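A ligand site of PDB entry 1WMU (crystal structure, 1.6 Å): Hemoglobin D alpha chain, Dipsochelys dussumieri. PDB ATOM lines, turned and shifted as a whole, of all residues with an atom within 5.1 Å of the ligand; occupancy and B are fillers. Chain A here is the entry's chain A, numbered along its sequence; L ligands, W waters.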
ATOM      1  N   MET A  32      -6.165  18.817  -7.948  1.00  0.00           N
ATOM      2  CA  MET A  32      -6.830  19.996  -7.379  1.00  0.00           C
ATOM      3  C   MET A  32      -7.259  20.951  -8.501  1.00  0.00           C
ATOM      4  O   MET A  32      -8.401  21.431  -8.519  1.00  0.00           O
ATOM      5  CB  MET A  32      -5.913  20.740  -6.402  1.00  0.00           C
ATOM      6  CG  MET A  32      -6.572  21.949  -5.721  1.00  0.00           C
ATOM      7  SD  MET A  32      -5.525  22.850  -4.563  1.00  0.00           S
ATOM      8  CE  MET A  32      -4.339  23.578  -5.686  1.00  0.00           C
ATOM      9  N   THR A  39      -9.228  26.887  -7.929  1.00  0.00           N
ATOM     10  CA  THR A  39      -7.889  26.983  -7.336  1.00  0.00           C
ATOM     11  C   THR A  39      -6.808  27.392  -8.342  1.00  0.00           C
ATOM     12  O   THR A  39      -5.744  27.866  -7.950  1.00  0.00           O
ATOM     13  CB  THR A  39      -7.461  25.653  -6.670  1.00  0.00           C
ATOM     14  OG1 THR A  39      -7.400  24.602  -7.646  1.00  0.00           O
ATOM     15  CG2 THR A  39      -8.459  25.269  -5.592  1.00  0.00           C
ATOM     16  N   TYR A  42      -4.912  30.970  -8.490  1.00  0.00           N
ATOM     17  CA  TYR A  42      -3.806  31.328  -7.595  1.00  0.00           C
ATOM     18  C   TYR A  42      -2.490  31.150  -8.348  1.00  0.00           C
ATOM     19  O   TYR A  42      -1.445  31.594  -7.888  1.00  0.00           O
ATOM     20  CB  TYR A  42      -3.791  30.390  -6.379  1.00  0.00           C
ATOM     21  CG  TYR A  42      -4.805  30.730  -5.324  1.00  0.00           C
ATOM     22  CD1 TYR A  42      -4.501  31.632  -4.304  1.00  0.00           C
ATOM     23  CD2 TYR A  42      -6.076  30.141  -5.324  1.00  0.00           C
ATOM     24  CE1 TYR A  42      -5.434  31.931  -3.309  1.00  0.00           C
ATOM     25  CE2 TYR A  42      -7.009  30.440  -4.328  1.00  0.00           C
ATOM     26  CZ  TYR A  42      -6.674  31.337  -3.329  1.00  0.00           C
ATOM     27  OH  TYR A  42      -7.561  31.610  -2.310  1.00  0.00           O
ATOM     28  N   PHE A  43      -2.566  30.491  -9.499  1.00  0.00           N
ATOM     29  CA  PHE A  43      -1.375  30.213 -10.305  1.00  0.00           C
ATOM     30  C   PHE A  43      -1.435  30.746 -11.743  1.00  0.00           C
ATOM     31  O   PHE A  43      -1.133  30.020 -12.687  1.00  0.00           O
ATOM     32  CB  PHE A  43      -1.111  28.710 -10.357  1.00  0.00           C
ATOM     33  CG  PHE A  43      -0.871  28.081  -9.015  1.00  0.00           C
ATOM     34  CD1 PHE A  43      -1.935  27.721  -8.197  1.00  0.00           C
ATOM     35  CD2 PHE A  43       0.420  27.824  -8.568  1.00  0.00           C
ATOM     36  CE1 PHE A  43      -1.721  27.121  -6.962  1.00  0.00           C
ATOM     37  CE2 PHE A  43       0.651  27.219  -7.337  1.00  0.00           C
ATOM     38  CZ  PHE A  43      -0.421  26.859  -6.525  1.00  0.00           C
ATOM     39  N   HIS A  45       0.528  32.688 -13.158  1.00  0.00           N
ATOM     40  CA  HIS A  45       1.894  32.749 -13.687  1.00  0.00           C
ATOM     41  C   HIS A  45       2.437  31.390 -14.110  1.00  0.00           C
ATOM     42  O   HIS A  45       3.516  31.300 -14.702  1.00  0.00           O
ATOM     43  CB  HIS A  45       2.826  33.387 -12.648  1.00  0.00           C
ATOM     44  CG  HIS A  45       2.768  32.735 -11.299  1.00  0.00           C
ATOM     45  ND1 HIS A  45       1.590  32.595 -10.585  1.00  0.00           N
ATOM     46  CD2 HIS A  45       3.743  32.221 -10.511  1.00  0.00           C
ATOM     47  CE1 HIS A  45       1.859  32.047  -9.416  1.00  0.00           C
ATOM     48  NE2 HIS A  45       3.151  31.810  -9.350  1.00  0.00           N
ATOM     49  N   PHE A  46       1.692  30.324 -13.799  1.00  0.00           N
ATOM     50  CA  PHE A  46       2.084  28.953 -14.139  1.00  0.00           C
ATOM     51  C   PHE A  46       1.480  28.435 -15.436  1.00  0.00           C
ATOM     52  O   PHE A  46       0.346  28.741 -15.775  1.00  0.00           O
ATOM     53  CB  PHE A  46       1.624  27.973 -13.064  1.00  0.00           C
ATOM     54  CG  PHE A  46       2.568  27.791 -11.918  1.00  0.00           C
ATOM     55  CD1 PHE A  46       3.357  28.837 -11.458  1.00  0.00           C
ATOM     56  CD2 PHE A  46       2.605  26.579 -11.235  1.00  0.00           C
ATOM     57  CE1 PHE A  46       4.172  28.680 -10.349  1.00  0.00           C
ATOM     58  CE2 PHE A  46       3.408  26.414 -10.112  1.00  0.00           C
ATOM     59  CZ  PHE A  46       4.196  27.464  -9.666  1.00  0.00           C
ATOM     60  N   HIS A  58       7.050  22.854  -8.410  1.00  0.00           N
ATOM     61  CA  HIS A  58       6.265  23.319  -7.270  1.00  0.00           C
ATOM     62  C   HIS A  58       5.745  22.102  -6.498  1.00  0.00           C
ATOM     63  O   HIS A  58       5.691  22.113  -5.267  1.00  0.00           O
ATOM     64  CB  HIS A  58       5.090  24.176  -7.735  1.00  0.00           C
ATOM     65  CG  HIS A  58       4.294  24.739  -6.601  1.00  0.00           C
ATOM     66  ND1 HIS A  58       4.869  25.481  -5.597  1.00  0.00           N
ATOM     67  CD2 HIS A  58       2.979  24.627  -6.294  1.00  0.00           C
ATOM     68  CE1 HIS A  58       3.949  25.799  -4.709  1.00  0.00           C
ATOM     69  NE2 HIS A  58       2.791  25.294  -5.099  1.00  0.00           N
ATOM     70  N   LYS A  61       8.278  21.071  -4.192  1.00  0.00           N
ATOM     71  CA  LYS A  61       8.399  21.988  -3.071  1.00  0.00           C
ATOM     72  C   LYS A  61       7.309  21.741  -2.029  1.00  0.00           C
ATOM     73  O   LYS A  61       7.560  21.776  -0.829  1.00  0.00           O
ATOM     74  CB  LYS A  61       8.314  23.441  -3.570  1.00  0.00           C
ATOM     75  CG  LYS A  61       9.519  23.915  -4.357  1.00  0.00           C
ATOM     76  CD  LYS A  61      10.693  24.229  -3.431  1.00  0.00           C
ATOM     77  CE  LYS A  61      11.857  24.847  -4.190  1.00  0.00           C
ATOM     78  NZ  LYS A  61      12.972  25.206  -3.258  1.00  0.00           N
ATOM     79  N   VAL A  62       6.086  21.511  -2.507  1.00  0.00           N
ATOM     80  CA  VAL A  62       4.981  21.256  -1.584  1.00  0.00           C
ATOM     81  C   VAL A  62       5.273  20.005  -0.766  1.00  0.00           C
ATOM     82  O   VAL A  62       5.138  20.011   0.466  1.00  0.00           O
ATOM     83  CB  VAL A  62       3.651  21.079  -2.352  1.00  0.00           C
ATOM     84  CG1 VAL A  62       2.525  20.692  -1.386  1.00  0.00           C
ATOM     85  CG2 VAL A  62       3.303  22.391  -3.048  1.00  0.00           C
ATOM     86  N   ALA A  65       7.953  20.536   1.849  1.00  0.00           N
ATOM     87  CA  ALA A  65       7.450  21.249   3.022  1.00  0.00           C
ATOM     88  C   ALA A  65       6.671  20.298   3.930  1.00  0.00           C
ATOM     89  O   ALA A  65       6.778  20.386   5.157  1.00  0.00           O
ATOM     90  CB  ALA A  65       6.559  22.418   2.602  1.00  0.00           C
ATOM     91  N   LEU A  66       5.886  19.410   3.339  1.00  0.00           N
ATOM     92  CA  LEU A  66       5.122  18.451   4.123  1.00  0.00           C
ATOM     93  C   LEU A  66       6.108  17.500   4.806  1.00  0.00           C
ATOM     94  O   LEU A  66       5.871  17.055   5.928  1.00  0.00           O
ATOM     95  CB  LEU A  66       4.161  17.664   3.228  1.00  0.00           C
ATOM     96  CG  LEU A  66       2.943  18.448   2.710  1.00  0.00           C
ATOM     97  CD1 LEU A  66       2.117  17.572   1.785  1.00  0.00           C
ATOM     98  CD2 LEU A  66       2.093  18.909   3.893  1.00  0.00           C
ATOM     99  N   LEU A  83       6.191  29.912   5.819  1.00  0.00           N
ATOM    100  CA  LEU A  83       5.156  29.518   4.874  1.00  0.00           C
ATOM    101  C   LEU A  83       3.771  30.012   5.286  1.00  0.00           C
ATOM    102  O   LEU A  83       2.938  30.301   4.420  1.00  0.00           O
ATOM    103  CB  LEU A  83       5.139  27.996   4.702  1.00  0.00           C
ATOM    104  CG  LEU A  83       6.358  27.442   3.951  1.00  0.00           C
ATOM    105  CD1 LEU A  83       6.299  25.919   3.903  1.00  0.00           C
ATOM    106  CD2 LEU A  83       6.398  28.035   2.564  1.00  0.00           C
ATOM    107  N   LEU A  86       3.600  33.531   4.251  1.00  0.00           N
ATOM    108  CA  LEU A  86       3.486  33.585   2.800  1.00  0.00           C
ATOM    109  C   LEU A  86       2.064  33.344   2.321  1.00  0.00           C
ATOM    110  O   LEU A  86       1.499  34.124   1.542  1.00  0.00           O
ATOM    111  CB  LEU A  86       4.402  32.544   2.168  1.00  0.00           C
ATOM    112  CG  LEU A  86       4.378  32.502   0.632  1.00  0.00           C
ATOM    113  CD1 LEU A  86       5.130  33.708   0.081  1.00  0.00           C
ATOM    114  CD2 LEU A  86       5.006  31.217   0.141  1.00  0.00           C
ATOM    115  N   HIS A  87       1.455  32.261   2.781  1.00  0.00           N
ATOM    116  CA  HIS A  87       0.109  31.932   2.341  1.00  0.00           C
ATOM    117  C   HIS A  87      -0.978  32.873   2.807  1.00  0.00           C
ATOM    118  O   HIS A  87      -1.962  33.089   2.101  1.00  0.00           O
ATOM    119  CB  HIS A  87      -0.236  30.485   2.694  1.00  0.00           C
ATOM    120  CG  HIS A  87       0.503  29.470   1.884  1.00  0.00           C
ATOM    121  ND1 HIS A  87       1.824  29.158   2.132  1.00  0.00           N
ATOM    122  CD2 HIS A  87       0.139  28.762   0.790  1.00  0.00           C
ATOM    123  CE1 HIS A  87       2.241  28.295   1.214  1.00  0.00           C
ATOM    124  NE2 HIS A  87       1.238  28.034   0.395  1.00  0.00           N
ATOM    125  N   LEU A  91      -0.108  35.550  -0.437  1.00  0.00           N
ATOM    126  CA  LEU A  91      -1.027  34.840  -1.321  1.00  0.00           C
ATOM    127  C   LEU A  91      -2.510  34.939  -0.981  1.00  0.00           C
ATOM    128  O   LEU A  91      -3.361  34.731  -1.840  1.00  0.00           O
ATOM    129  CB  LEU A  91      -0.611  33.369  -1.382  1.00  0.00           C
ATOM    130  CG  LEU A  91       0.854  33.126  -1.771  1.00  0.00           C
ATOM    131  CD1 LEU A  91       1.230  31.682  -1.499  1.00  0.00           C
ATOM    132  CD2 LEU A  91       1.068  33.485  -3.244  1.00  0.00           C
ATOM    133  N   VAL A  93      -4.452  32.967   0.637  1.00  0.00           N
ATOM    134  CA  VAL A  93      -5.145  31.732   0.302  1.00  0.00           C
ATOM    135  C   VAL A  93      -6.360  31.494   1.198  1.00  0.00           C
ATOM    136  O   VAL A  93      -6.277  31.563   2.423  1.00  0.00           O
ATOM    137  CB  VAL A  93      -4.187  30.523   0.388  1.00  0.00           C
ATOM    138  CG1 VAL A  93      -4.937  29.240   0.104  1.00  0.00           C
ATOM    139  CG2 VAL A  93      -3.060  30.686  -0.632  1.00  0.00           C
ATOM    140  N   ASN A  97      -9.339  26.158   0.609  1.00  0.00           N
ATOM    141  CA  ASN A  97      -8.440  25.520  -0.337  1.00  0.00           C
ATOM    142  C   ASN A  97      -7.391  24.604   0.274  1.00  0.00           C
ATOM    143  O   ASN A  97      -6.913  23.685  -0.393  1.00  0.00           O
ATOM    144  CB  ASN A  97      -7.802  26.582  -1.223  1.00  0.00           C
ATOM    145  CG  ASN A  97      -8.828  27.287  -2.065  1.00  0.00           C
ATOM    146  OD1 ASN A  97      -9.753  26.659  -2.581  1.00  0.00           O
ATOM    147  ND2 ASN A  97      -8.688  28.604  -2.209  1.00  0.00           N
ATOM    148  N   PHE A  98      -7.020  24.859   1.527  1.00  0.00           N
ATOM    149  CA  PHE A  98      -6.051  23.979   2.181  1.00  0.00           C
ATOM    150  C   PHE A  98      -6.712  22.615   2.315  1.00  0.00           C
ATOM    151  O   PHE A  98      -6.064  21.576   2.157  1.00  0.00           O
ATOM    152  CB  PHE A  98      -5.662  24.520   3.556  1.00  0.00           C
ATOM    153  CG  PHE A  98      -4.839  25.768   3.500  1.00  0.00           C
ATOM    154  CD1 PHE A  98      -3.656  25.804   2.769  1.00  0.00           C
ATOM    155  CD2 PHE A  98      -5.240  26.920   4.176  1.00  0.00           C
ATOM    156  CE1 PHE A  98      -2.887  26.966   2.716  1.00  0.00           C
ATOM    157  CE2 PHE A  98      -4.484  28.078   4.123  1.00  0.00           C
ATOM    158  CZ  PHE A  98      -3.298  28.105   3.389  1.00  0.00           C
ATOM    159  N   LEU A 101      -6.645  20.828  -1.178  1.00  0.00           N
ATOM    160  CA  LEU A 101      -5.346  20.237  -1.519  1.00  0.00           C
ATOM    161  C   LEU A 101      -5.074  19.028  -0.619  1.00  0.00           C
ATOM    162  O   LEU A 101      -4.560  18.016  -1.080  1.00  0.00           O
ATOM    163  CB  LEU A 101      -4.214  21.267  -1.389  1.00  0.00           C
ATOM    164  CG  LEU A 101      -2.821  20.729  -1.763  1.00  0.00           C
ATOM    165  CD1 LEU A 101      -2.861  20.126  -3.170  1.00  0.00           C
ATOM    166  CD2 LEU A 101      -1.809  21.864  -1.698  1.00  0.00           C
ATOM    167  N   SER A 102      -5.441  19.150   0.662  1.00  0.00           N
ATOM    168  CA  SER A 102      -5.256  18.045   1.598  1.00  0.00           C
ATOM    169  C   SER A 102      -6.023  16.823   1.089  1.00  0.00           C
ATOM    170  O   SER A 102      -5.498  15.716   1.074  1.00  0.00           O
ATOM    171  CB  SER A 102      -5.765  18.438   2.986  1.00  0.00           C
ATOM    172  OG  SER A 102      -4.904  19.390   3.595  1.00  0.00           O
ATOM    173  N   VAL A 132      -1.371  20.735   9.613  1.00  0.00           N
ATOM    174  CA  VAL A 132      -0.549  21.562   8.751  1.00  0.00           C
ATOM    175  C   VAL A 132      -1.392  22.714   8.202  1.00  0.00           C
ATOM    176  O   VAL A 132      -0.946  23.861   8.169  1.00  0.00           O
ATOM    177  CB  VAL A 132       0.010  20.750   7.563  1.00  0.00           C
ATOM    178  CG1 VAL A 132       0.676  21.675   6.557  1.00  0.00           C
ATOM    179  CG2 VAL A 132       1.026  19.724   8.078  1.00  0.00           C
ATOM    180  N   LEU A 136      -0.874  26.830   8.410  1.00  0.00           N
ATOM    181  CA  LEU A 136      -0.722  27.676   7.235  1.00  0.00           C
ATOM    182  C   LEU A 136      -1.765  28.787   7.189  1.00  0.00           C
ATOM    183  O   LEU A 136      -1.611  29.737   6.418  1.00  0.00           O
ATOM    184  CB  LEU A 136      -0.782  26.831   5.965  1.00  0.00           C
ATOM    185  CG  LEU A 136       0.415  25.894   5.784  1.00  0.00           C
ATOM    186  CD1 LEU A 136       0.214  25.071   4.538  1.00  0.00           C
ATOM    187  CD2 LEU A 136       1.700  26.700   5.685  1.00  0.00           C
HETATM  188  C1  LIG L   1       3.911  28.360  -2.688  1.00  0.00           C
HETATM  189  C2  LIG L   1       3.539  24.837   0.624  1.00  0.00           C
HETATM  190  C3  LIG L   1      -1.318  24.916   0.020  1.00  0.00           C
HETATM  191  C4  LIG L   1      -0.958  28.427  -3.368  1.00  0.00           C
HETATM  192  C5  LIG L   1       4.206  27.417  -1.731  1.00  0.00           C
HETATM  193  C6  LIG L   1       5.558  27.115  -1.290  1.00  0.00           C
HETATM  194  C7  LIG L   1       5.463  26.106  -0.358  1.00  0.00           C
HETATM  195  C8  LIG L   1       4.061  25.802  -0.218  1.00  0.00           C
HETATM  196  C9  LIG L   1       6.604  25.431   0.382  1.00  0.00           C
HETATM  197  C10 LIG L   1       6.804  27.811  -1.813  1.00  0.00           C
HETATM  198  C11 LIG L   1       7.502  27.138  -3.013  1.00  0.00           C
HETATM  199  C12 LIG L   1       8.821  27.830  -3.359  1.00  0.00           C
HETATM  200  O1  LIG L   1       9.486  28.348  -2.420  1.00  0.00           O
HETATM  201  O2  LIG L   1       9.135  27.826  -4.553  1.00  0.00           O
HETATM  202  C13 LIG L   1       2.176  24.568   0.733  1.00  0.00           C
HETATM  203  C14 LIG L   1       1.625  23.559   1.610  1.00  0.00           C
HETATM  204  C15 LIG L   1       0.254  23.582   1.444  1.00  0.00           C
HETATM  205  C16 LIG L   1      -0.038  24.605   0.452  1.00  0.00           C
HETATM  206  C17 LIG L   1       2.448  22.663   2.523  1.00  0.00           C
HETATM  207  C18 LIG L   1      -0.798  22.718   2.129  1.00  0.00           C
HETATM  208  C19 LIG L   1      -0.673  21.218   1.902  1.00  0.00           C
HETATM  209  C20 LIG L   1      -1.621  25.864  -0.926  1.00  0.00           C
HETATM  210  C21 LIG L   1      -2.975  26.130  -1.362  1.00  0.00           C
HETATM  211  C22 LIG L   1      -2.876  27.119  -2.331  1.00  0.00           C
HETATM  212  C23 LIG L   1      -1.475  27.473  -2.486  1.00  0.00           C
HETATM  213  C24 LIG L   1      -4.204  25.403  -0.829  1.00  0.00           C
HETATM  214  C25 LIG L   1      -4.028  27.740  -3.116  1.00  0.00           C
HETATM  215  C26 LIG L   1      -4.825  26.984  -3.910  1.00  0.00           C
HETATM  216  C27 LIG L   1       0.415  28.710  -3.473  1.00  0.00           C
HETATM  217  C28 LIG L   1       1.005  29.669  -4.393  1.00  0.00           C
HETATM  218  C29 LIG L   1       2.368  29.646  -4.204  1.00  0.00           C
HETATM  219  C30 LIG L   1       2.631  28.670  -3.149  1.00  0.00           C
HETATM  220  C31 LIG L   1       0.281  30.531  -5.403  1.00  0.00           C
HETATM  221  C32 LIG L   1       3.421  30.460  -4.964  1.00  0.00           C
HETATM  222  C33 LIG L   1       4.409  29.511  -5.696  1.00  0.00           C
HETATM  223  C34 LIG L   1       5.172  30.028  -6.905  1.00  0.00           C
HETATM  224  O3  LIG L   1       4.948  31.193  -7.311  1.00  0.00           O
HETATM  225  O4  LIG L   1       5.965  29.205  -7.418  1.00  0.00           O
HETATM  226  N1  LIG L   1       3.353  26.624  -1.063  1.00  0.00           N
HETATM  227  N2  LIG L   1       1.140  25.161   0.074  1.00  0.00           N
HETATM  228  N3  LIG L   1      -0.763  26.683  -1.601  1.00  0.00           N
HETATM  229  N4  LIG L   1       1.445  28.141  -2.762  1.00  0.00           N
HETATM  230 FE1  LIG L   1       1.283  26.659  -1.296  1.00  0.00          FE
HETATM  231  O   HOH W   1       8.498  31.351  -1.181  1.00  0.00           O
HETATM  232  O   HOH W   2       7.563  28.796  -9.505  1.00  0.00           O
HETATM  233  O   HOH W   3       7.289  26.891  -6.285  1.00  0.00           O
HETATM  234  O   HOH W   4      10.045  25.842  -0.573  1.00  0.00           O
HETATM  235  O   HOH W   5       7.076  32.294  -8.415  1.00  0.00           O
HETATM  236  O   HOH W   6      11.680  29.769  -2.622  1.00  0.00           O
HETATM  237  O   HOH W   7       4.296  33.594  -6.223  1.00  0.00           O
HETATM  238  O   HOH W   8      11.442  28.233  -5.913  1.00  0.00           O
HETATM  239  O   HOH W   9       1.230  25.321  -2.769  1.00  0.00           O
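Water W3 bridges O2 of the ligand (2.7 Å) and ND1 of His 58 (2.9 Å).
Merely in contact with the ligand: Met 32 (3.9 Å), Tyr 42 (3.2 Å), Phe 43 (3.6 Å), Phe 46 (3.3 Å), His 58 (3.3 Å), Lys 61 (3.8 Å), Ala 65 (3.7 Å), Leu 83 (3.4 Å), Leu 91 (3.5 Å), Val 93 (3.7 Å), Asn 97 (3.2 Å), Phe 98 (3.7 Å), Leu 101 (3.5 Å) and Leu 136 (3.4 Å). Hydrophobic or aromatic side chains within 4 Å of the ligand: Met 32, Tyr 42, Phe 43, His 45, Phe 46, His 58, Ala 65, Leu 83, His 87, Leu 91, Val 93, Phe 98, Leu 101 and Leu 136. 16 residues have an atom within 4 Å of the ligand: Met 32, Tyr 42, Phe 43, His 45, Phe 46, His 58, Lys 61, Ala 65, Leu 83, His 87, Leu 91, Val 93, Asn 97, Phe 98, Leu 101 and Leu 136. The nearest printed residue that does not touch the ligand is Leu 66 (4.01 Å).
A ring nitrogen (ND1) of His 87 is in hydrogen-bond range of the backbone carbonyl oxygen of Leu 83 (2.8 Å). O of His 87 sits at hydrogen-bond distance from N of Val 93 (2.9 Å). The side-chain hydroxyl of Tyr 42 sits at hydrogen-bond distance from the side-chain amide nitrogen of Asn 97 (3.2 Å). N of Leu 91 lies within hydrogen-bond range of O of Leu 86 (2.9 Å). O of Phe 98 lies within hydrogen-bond range of OG of Ser 102 (2.9 Å). The backbone carbonyl oxygen (O) of Met 32 lies close to the side-chain hydroxyl (OG1) of Thr 39, at 3.4 Å.
NE2 of His 87 binds FE1 of the ligand. An oxygen (O3) of the ligand is in hydrogen-bond range of a ring nitrogen (NE2) of His 45 (2.8 Å).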
